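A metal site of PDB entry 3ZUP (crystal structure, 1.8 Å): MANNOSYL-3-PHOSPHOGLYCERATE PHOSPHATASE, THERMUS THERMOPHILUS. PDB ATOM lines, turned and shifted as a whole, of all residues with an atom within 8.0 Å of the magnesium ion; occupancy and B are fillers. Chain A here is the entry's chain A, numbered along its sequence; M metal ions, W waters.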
ATOM      1  N   THR A   5      26.489 -25.794  15.170  1.00  0.00           N
ATOM      2  CA  THR A   5      26.165 -26.617  14.010  1.00  0.00           C
ATOM      3  C   THR A   5      26.356 -25.913  12.693  1.00  0.00           C
ATOM      4  O   THR A   5      25.995 -24.748  12.503  1.00  0.00           O
ATOM      5  CB  THR A   5      24.727 -27.158  14.087  1.00  0.00           C
ATOM      6  OG1 THR A   5      24.523 -28.116  13.046  1.00  0.00           O
ATOM      7  CG2 THR A   5      23.700 -26.010  13.946  1.00  0.00           C
ATOM      8  N   ASP A   6      26.932 -26.653  11.765  1.00  0.00           N
ATOM      9  CA  ASP A   6      27.005 -26.231  10.389  1.00  0.00           C
ATOM     10  C   ASP A   6      25.572 -26.198   9.823  1.00  0.00           C
ATOM     11  O   ASP A   6      24.659 -26.789  10.419  1.00  0.00           O
ATOM     12  CB  ASP A   6      27.880 -27.250   9.680  1.00  0.00           C
ATOM     13  CG  ASP A   6      27.913 -27.052   8.204  1.00  0.00           C
ATOM     14  OD1 ASP A   6      28.163 -25.909   7.760  1.00  0.00           O
ATOM     15  OD2 ASP A   6      27.673 -28.047   7.498  1.00  0.00           O
ATOM     16  N   LEU A   7      25.368 -25.490   8.714  1.00  0.00           N
ATOM     17  CA  LEU A   7      24.040 -25.425   8.114  1.00  0.00           C
ATOM     18  C   LEU A   7      23.876 -26.372   6.917  1.00  0.00           C
ATOM     19  O   LEU A   7      23.293 -27.452   7.060  1.00  0.00           O
ATOM     20  CB  LEU A   7      23.628 -23.974   7.795  1.00  0.00           C
ATOM     21  CG  LEU A   7      23.417 -23.052   9.001  1.00  0.00           C
ATOM     22  CD1 LEU A   7      23.019 -21.621   8.535  1.00  0.00           C
ATOM     23  CD2 LEU A   7      22.356 -23.615   9.919  1.00  0.00           C
ATOM     24  N   ASP A   8      24.409 -25.988   5.755  1.00  0.00           N
ATOM     25  CA  ASP A   8      24.243 -26.787   4.536  1.00  0.00           C
ATOM     26  C   ASP A   8      24.943 -28.128   4.637  1.00  0.00           C
ATOM     27  O   ASP A   8      26.125 -28.193   4.917  1.00  0.00           O
ATOM     28  CB  ASP A   8      24.770 -26.051   3.289  1.00  0.00           C
ATOM     29  CG  ASP A   8      23.884 -24.893   2.877  1.00  0.00           C
ATOM     30  OD1 ASP A   8      22.759 -24.771   3.415  1.00  0.00           O
ATOM     31  OD2 ASP A   8      24.307 -24.101   2.002  1.00  0.00           O
ATOM     32  N   GLY A   9      24.206 -29.204   4.392  1.00  0.00           N
ATOM     33  CA  GLY A   9      24.778 -30.547   4.487  1.00  0.00           C
ATOM     34  C   GLY A   9      24.738 -31.135   5.888  1.00  0.00           C
ATOM     35  O   GLY A   9      25.076 -32.302   6.095  1.00  0.00           O
ATOM     36  N   THR A  10      24.341 -30.327   6.873  1.00  0.00           N
ATOM     37  CA  THR A  10      24.293 -30.803   8.251  1.00  0.00           C
ATOM     38  C   THR A  10      22.874 -30.653   8.791  1.00  0.00           C
ATOM     39  O   THR A  10      22.158 -31.640   8.970  1.00  0.00           O
ATOM     40  CB  THR A  10      25.311 -30.064   9.141  1.00  0.00           C
ATOM     41  OG1 THR A  10      26.631 -30.378   8.686  1.00  0.00           O
ATOM     42  CG2 THR A  10      25.199 -30.472  10.607  1.00  0.00           C
ATOM     43  N   LEU A  11      22.482 -29.407   9.002  1.00  0.00           N
ATOM     44  CA  LEU A  11      21.130 -29.075   9.452  1.00  0.00           C
ATOM     45  C   LEU A  11      20.124 -28.999   8.295  1.00  0.00           C
ATOM     46  O   LEU A  11      18.938 -29.289   8.473  1.00  0.00           O
ATOM     47  CB  LEU A  11      21.176 -27.765  10.232  1.00  0.00           C
ATOM     48  CG  LEU A  11      19.958 -27.375  11.064  1.00  0.00           C
ATOM     49  CD1 LEU A  11      19.534 -28.531  11.955  1.00  0.00           C
ATOM     50  CD2 LEU A  11      20.271 -26.136  11.893  1.00  0.00           C
ATOM     51  N   LEU A  12      20.599 -28.624   7.102  1.00  0.00           N
ATOM     52  CA  LEU A  12      19.734 -28.466   5.940  1.00  0.00           C
ATOM     53  C   LEU A  12      20.125 -29.445   4.847  1.00  0.00           C
ATOM     54  O   LEU A  12      21.306 -29.726   4.669  1.00  0.00           O
ATOM     55  CB  LEU A  12      19.853 -27.053   5.367  1.00  0.00           C
ATOM     56  CG  LEU A  12      19.627 -25.930   6.365  1.00  0.00           C
ATOM     57  CD1 LEU A  12      19.814 -24.586   5.687  1.00  0.00           C
ATOM     58  CD2 LEU A  12      18.245 -26.066   6.957  1.00  0.00           C
ATOM     59  N   VAL A  38      27.080 -22.165  12.731  1.00  0.00           N
ATOM     60  CA  VAL A  38      28.478 -21.833  12.450  1.00  0.00           C
ATOM     61  C   VAL A  38      28.665 -22.214  10.994  1.00  0.00           C
ATOM     62  O   VAL A  38      28.769 -23.382  10.660  1.00  0.00           O
ATOM     63  CB  VAL A  38      29.448 -22.634  13.351  1.00  0.00           C
ATOM     64  CG1 VAL A  38      30.892 -22.136  13.125  1.00  0.00           C
ATOM     65  CG2 VAL A  38      29.064 -22.483  14.838  1.00  0.00           C
ATOM     66  N   THR A  39      28.683 -21.209  10.114  1.00  0.00           N
ATOM     67  CA  THR A  39      28.400 -21.447   8.712  1.00  0.00           C
ATOM     68  C   THR A  39      29.390 -20.678   7.818  1.00  0.00           C
ATOM     69  O   THR A  39      30.016 -19.718   8.277  1.00  0.00           O
ATOM     70  CB  THR A  39      26.947 -20.998   8.390  1.00  0.00           C
ATOM     71  OG1 THR A  39      26.622 -21.218   7.017  1.00  0.00           O
ATOM     72  CG2 THR A  39      26.726 -19.538   8.731  1.00  0.00           C
ATOM     73  N   ALA A  40      29.523 -21.127   6.563  1.00  0.00           N
ATOM     74  CA  ALA A  40      30.231 -20.379   5.519  1.00  0.00           C
ATOM     75  C   ALA A  40      29.347 -19.234   4.981  1.00  0.00           C
ATOM     76  O   ALA A  40      29.834 -18.347   4.258  1.00  0.00           O
ATOM     77  CB  ALA A  40      30.591 -21.314   4.379  1.00  0.00           C
ATOM     78  N   LYS A  41      28.057 -19.302   5.280  1.00  0.00           N
ATOM     79  CA  LYS A  41      27.091 -18.323   4.778  1.00  0.00           C
ATOM     80  C   LYS A  41      27.310 -16.924   5.339  1.00  0.00           C
ATOM     81  O   LYS A  41      27.902 -16.735   6.416  1.00  0.00           O
ATOM     82  CB  LYS A  41      25.652 -18.744   5.089  1.00  0.00           C
ATOM     83  CG  LYS A  41      25.197 -19.991   4.318  1.00  0.00           C
ATOM     84  CD  LYS A  41      23.785 -20.403   4.759  1.00  0.00           C
ATOM     85  CE  LYS A  41      23.400 -21.746   4.162  1.00  0.00           C
ATOM     86  NZ  LYS A  41      23.265 -21.698   2.683  1.00  0.00           N
ATOM     87  N   HIS A 164      37.615 -25.455   2.333  1.00  0.00           N
ATOM     88  CA  HIS A 164      36.657 -25.955   1.351  1.00  0.00           C
ATOM     89  C   HIS A 164      35.353 -26.201   2.102  1.00  0.00           C
ATOM     90  O   HIS A 164      35.379 -26.746   3.208  1.00  0.00           O
ATOM     91  CB  HIS A 164      37.181 -27.255   0.758  1.00  0.00           C
ATOM     92  CG  HIS A 164      36.366 -27.809  -0.361  1.00  0.00           C
ATOM     93  ND1 HIS A 164      35.359 -28.740  -0.173  1.00  0.00           N
ATOM     94  CD2 HIS A 164      36.433 -27.614  -1.699  1.00  0.00           C
ATOM     95  CE1 HIS A 164      34.834 -29.074  -1.329  1.00  0.00           C
ATOM     96  NE2 HIS A 164      35.475 -28.415  -2.285  1.00  0.00           N
ATOM     97  N   GLY A 165      34.232 -25.780   1.534  1.00  0.00           N
ATOM     98  CA  GLY A 165      32.981 -25.799   2.275  1.00  0.00           C
ATOM     99  C   GLY A 165      32.035 -26.923   1.891  1.00  0.00           C
ATOM    100  O   GLY A 165      30.931 -27.020   2.420  1.00  0.00           O
ATOM    101  N   GLY A 166      32.489 -27.798   0.987  1.00  0.00           N
ATOM    102  CA  GLY A 166      31.643 -28.900   0.525  1.00  0.00           C
ATOM    103  C   GLY A 166      31.524 -28.894  -0.985  1.00  0.00           C
ATOM    104  O   GLY A 166      31.534 -29.961  -1.617  1.00  0.00           O
ATOM    105  N   ARG A 167      31.424 -27.696  -1.565  1.00  0.00           N
ATOM    106  CA  ARG A 167      31.424 -27.558  -3.021  1.00  0.00           C
ATOM    107  C   ARG A 167      32.475 -26.561  -3.529  1.00  0.00           C
ATOM    108  O   ARG A 167      33.087 -26.775  -4.586  1.00  0.00           O
ATOM    109  CB  ARG A 167      30.061 -27.145  -3.569  1.00  0.00           C
ATOM    110  CG  ARG A 167      30.177 -26.679  -5.022  1.00  0.00           C
ATOM    111  CD  ARG A 167      28.866 -26.648  -5.767  1.00  0.00           C
ATOM    112  NE  ARG A 167      29.088 -26.257  -7.150  1.00  0.00           N
ATOM    113  CZ  ARG A 167      28.139 -26.198  -8.083  1.00  0.00           C
ATOM    114  NH1 ARG A 167      26.885 -26.509  -7.750  1.00  0.00           N
ATOM    115  NH2 ARG A 167      28.439 -25.833  -9.319  1.00  0.00           N
ATOM    116  N   LYS A 177      36.451 -21.618  11.822  1.00  0.00           N
ATOM    117  CA  LYS A 177      35.245 -21.943  12.611  1.00  0.00           C
ATOM    118  C   LYS A 177      35.629 -22.275  14.059  1.00  0.00           C
ATOM    119  O   LYS A 177      34.885 -21.971  14.975  1.00  0.00           O
ATOM    120  CB  LYS A 177      34.452 -23.096  11.992  1.00  0.00           C
ATOM    121  CG  LYS A 177      33.620 -22.709  10.759  1.00  0.00           C
ATOM    122  CD  LYS A 177      32.643 -23.816  10.371  1.00  0.00           C
ATOM    123  CE  LYS A 177      31.841 -23.440   9.129  1.00  0.00           C
ATOM    124  NZ  LYS A 177      30.813 -24.442   8.815  1.00  0.00           N
ATOM    125  N   LEU A 200      28.559 -30.145  15.150  1.00  0.00           N
ATOM    126  CA  LEU A 200      28.113 -31.035  14.080  1.00  0.00           C
ATOM    127  C   LEU A 200      28.480 -30.395  12.753  1.00  0.00           C
ATOM    128  O   LEU A 200      28.309 -29.205  12.580  1.00  0.00           O
ATOM    129  CB  LEU A 200      26.593 -31.253  14.120  1.00  0.00           C
ATOM    130  CG  LEU A 200      26.073 -31.841  15.441  1.00  0.00           C
ATOM    131  CD1 LEU A 200      25.420 -30.786  16.304  1.00  0.00           C
ATOM    132  CD2 LEU A 200      25.134 -33.028  15.199  1.00  0.00           C
ATOM    133  N   GLY A 201      28.998 -31.186  11.813  1.00  0.00           N
ATOM    134  CA  GLY A 201      29.359 -30.623  10.527  1.00  0.00           C
ATOM    135  C   GLY A 201      29.607 -31.702   9.493  1.00  0.00           C
ATOM    136  O   GLY A 201      29.474 -32.888   9.792  1.00  0.00           O
ATOM    137  N   ASP A 202      29.996 -31.296   8.284  1.00  0.00           N
ATOM    138  CA  ASP A 202      30.081 -32.250   7.178  1.00  0.00           C
ATOM    139  C   ASP A 202      31.216 -32.024   6.179  1.00  0.00           C
ATOM    140  O   ASP A 202      31.377 -32.802   5.240  1.00  0.00           O
ATOM    141  CB  ASP A 202      28.730 -32.323   6.440  1.00  0.00           C
ATOM    142  CG  ASP A 202      28.560 -31.207   5.421  1.00  0.00           C
ATOM    143  OD1 ASP A 202      28.930 -30.059   5.730  1.00  0.00           O
ATOM    144  OD2 ASP A 202      28.081 -31.469   4.296  1.00  0.00           O
ATOM    145  N   SER A 203      32.010 -30.966   6.346  1.00  0.00           N
ATOM    146  CA  SER A 203      33.032 -30.669   5.346  1.00  0.00           C
ATOM    147  C   SER A 203      34.386 -30.246   5.941  1.00  0.00           C
ATOM    148  O   SER A 203      34.543 -30.126   7.153  1.00  0.00           O
ATOM    149  CB  SER A 203      32.538 -29.597   4.376  1.00  0.00           C
ATOM    150  OG  SER A 203      31.428 -30.069   3.629  1.00  0.00           O
ATOM    151  N   LEU A 204      35.353 -29.992   5.052  1.00  0.00           N
ATOM    152  CA  LEU A 204      36.699 -29.643   5.476  1.00  0.00           C
ATOM    153  C   LEU A 204      36.690 -28.453   6.416  1.00  0.00           C
ATOM    154  O   LEU A 204      37.421 -28.422   7.423  1.00  0.00           O
ATOM    155  CB  LEU A 204      37.582 -29.376   4.245  1.00  0.00           C
ATOM    156  CG  LEU A 204      39.020 -28.957   4.552  1.00  0.00           C
ATOM    157  CD1 LEU A 204      39.757 -30.081   5.297  1.00  0.00           C
ATOM    158  CD2 LEU A 204      39.774 -28.559   3.272  1.00  0.00           C
ATOM    159  N   ASN A 205      35.858 -27.461   6.114  1.00  0.00           N
ATOM    160  CA  ASN A 205      35.811 -26.240   6.914  1.00  0.00           C
ATOM    161  C   ASN A 205      35.244 -26.473   8.306  1.00  0.00           C
ATOM    162  O   ASN A 205      35.320 -25.578   9.136  1.00  0.00           O
ATOM    163  CB  ASN A 205      35.071 -25.086   6.191  1.00  0.00           C
ATOM    164  CG  ASN A 205      33.604 -25.400   5.916  1.00  0.00           C
ATOM    165  OD1 ASN A 205      33.203 -26.553   5.845  1.00  0.00           O
ATOM    166  ND2 ASN A 205      32.809 -24.354   5.717  1.00  0.00           N
ATOM    167  N   ASP A 206      34.716 -27.683   8.553  1.00  0.00           N
ATOM    168  CA  ASP A 206      34.222 -28.061   9.873  1.00  0.00           C
ATOM    169  C   ASP A 206      35.235 -28.787  10.743  1.00  0.00           C
ATOM    170  O   ASP A 206      34.991 -29.013  11.917  1.00  0.00           O
ATOM    171  CB  ASP A 206      32.948 -28.907   9.733  1.00  0.00           C
ATOM    172  CG  ASP A 206      31.841 -28.146   9.080  1.00  0.00           C
ATOM    173  OD1 ASP A 206      31.633 -26.966   9.477  1.00  0.00           O
ATOM    174  OD2 ASP A 206      31.217 -28.687   8.155  1.00  0.00           O
ATOM    175  N   VAL A 219      28.463 -35.617   9.984  1.00  0.00           N
ATOM    176  CA  VAL A 219      27.329 -36.128   9.236  1.00  0.00           C
ATOM    177  C   VAL A 219      27.526 -35.947   7.727  1.00  0.00           C
ATOM    178  O   VAL A 219      26.554 -35.888   6.962  1.00  0.00           O
ATOM    179  CB  VAL A 219      26.003 -35.485   9.696  1.00  0.00           C
ATOM    180  CG1 VAL A 219      25.794 -35.763  11.166  1.00  0.00           C
ATOM    181  CG2 VAL A 219      26.027 -33.969   9.430  1.00  0.00           C
HETATM  182 MG    MG M   1      28.232 -27.876   5.353  1.00  0.00          MG
HETATM  183  O   HOH W   1      28.691 -28.463   3.131  1.00  0.00           O
HETATM  184  O   HOH W   2      28.215 -25.750   4.436  1.00  0.00           O
HETATM  185  O   HOH W   3      30.482 -27.430   5.991  1.00  0.00           O
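The magnesium ion is bound by O of Asp 8 (2.2 Å), OD2 of Asp 6 (2.2 Å), water W2 (2.3 Å), OD1 of Asp 202 (2.3 Å), water W1 (2.3 Å) and water W3 (2.4 Å).
The side-chain carboxylate (OD2) of Asp 206 lies within hydrogen-bond range of the backbone NH (N) of Asp 202. The backbone NH of Asp 6 lies within hydrogen-bond range of the backbone carbonyl oxygen of Leu 200 (3.0 Å). The side-chain carboxylate (OD1) of Asp 6 is in salt-bridge range of the side-chain amino group (NZ) of Lys 177 (3.2 Å). NZ of Lys 41 lies within salt-bridge range of OD2 of Asp 8 (2.7 Å). The side-chain carboxylate (OD2) of Asp 6 sits close to the side-chain hydroxyl (OG1) of Thr 10, 2.8 Å away. The side-chain carboxylate of Asp 202 sits close to the side-chain hydroxyl of Ser 203, at 3.3 Å.
Within 4 Å of the magnesium ion: Asp 6, Asp 8 and Asp 202. The nearest printed residue that does not touch the magnesium ion is Gly 165 (4.1 Å).
Water W1 lies within hydrogen-bond range of O of Gly 165 (2.8 Å), OG of Ser 203 (3.2 Å) and OD2 of Asp 202 (3.3 Å).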
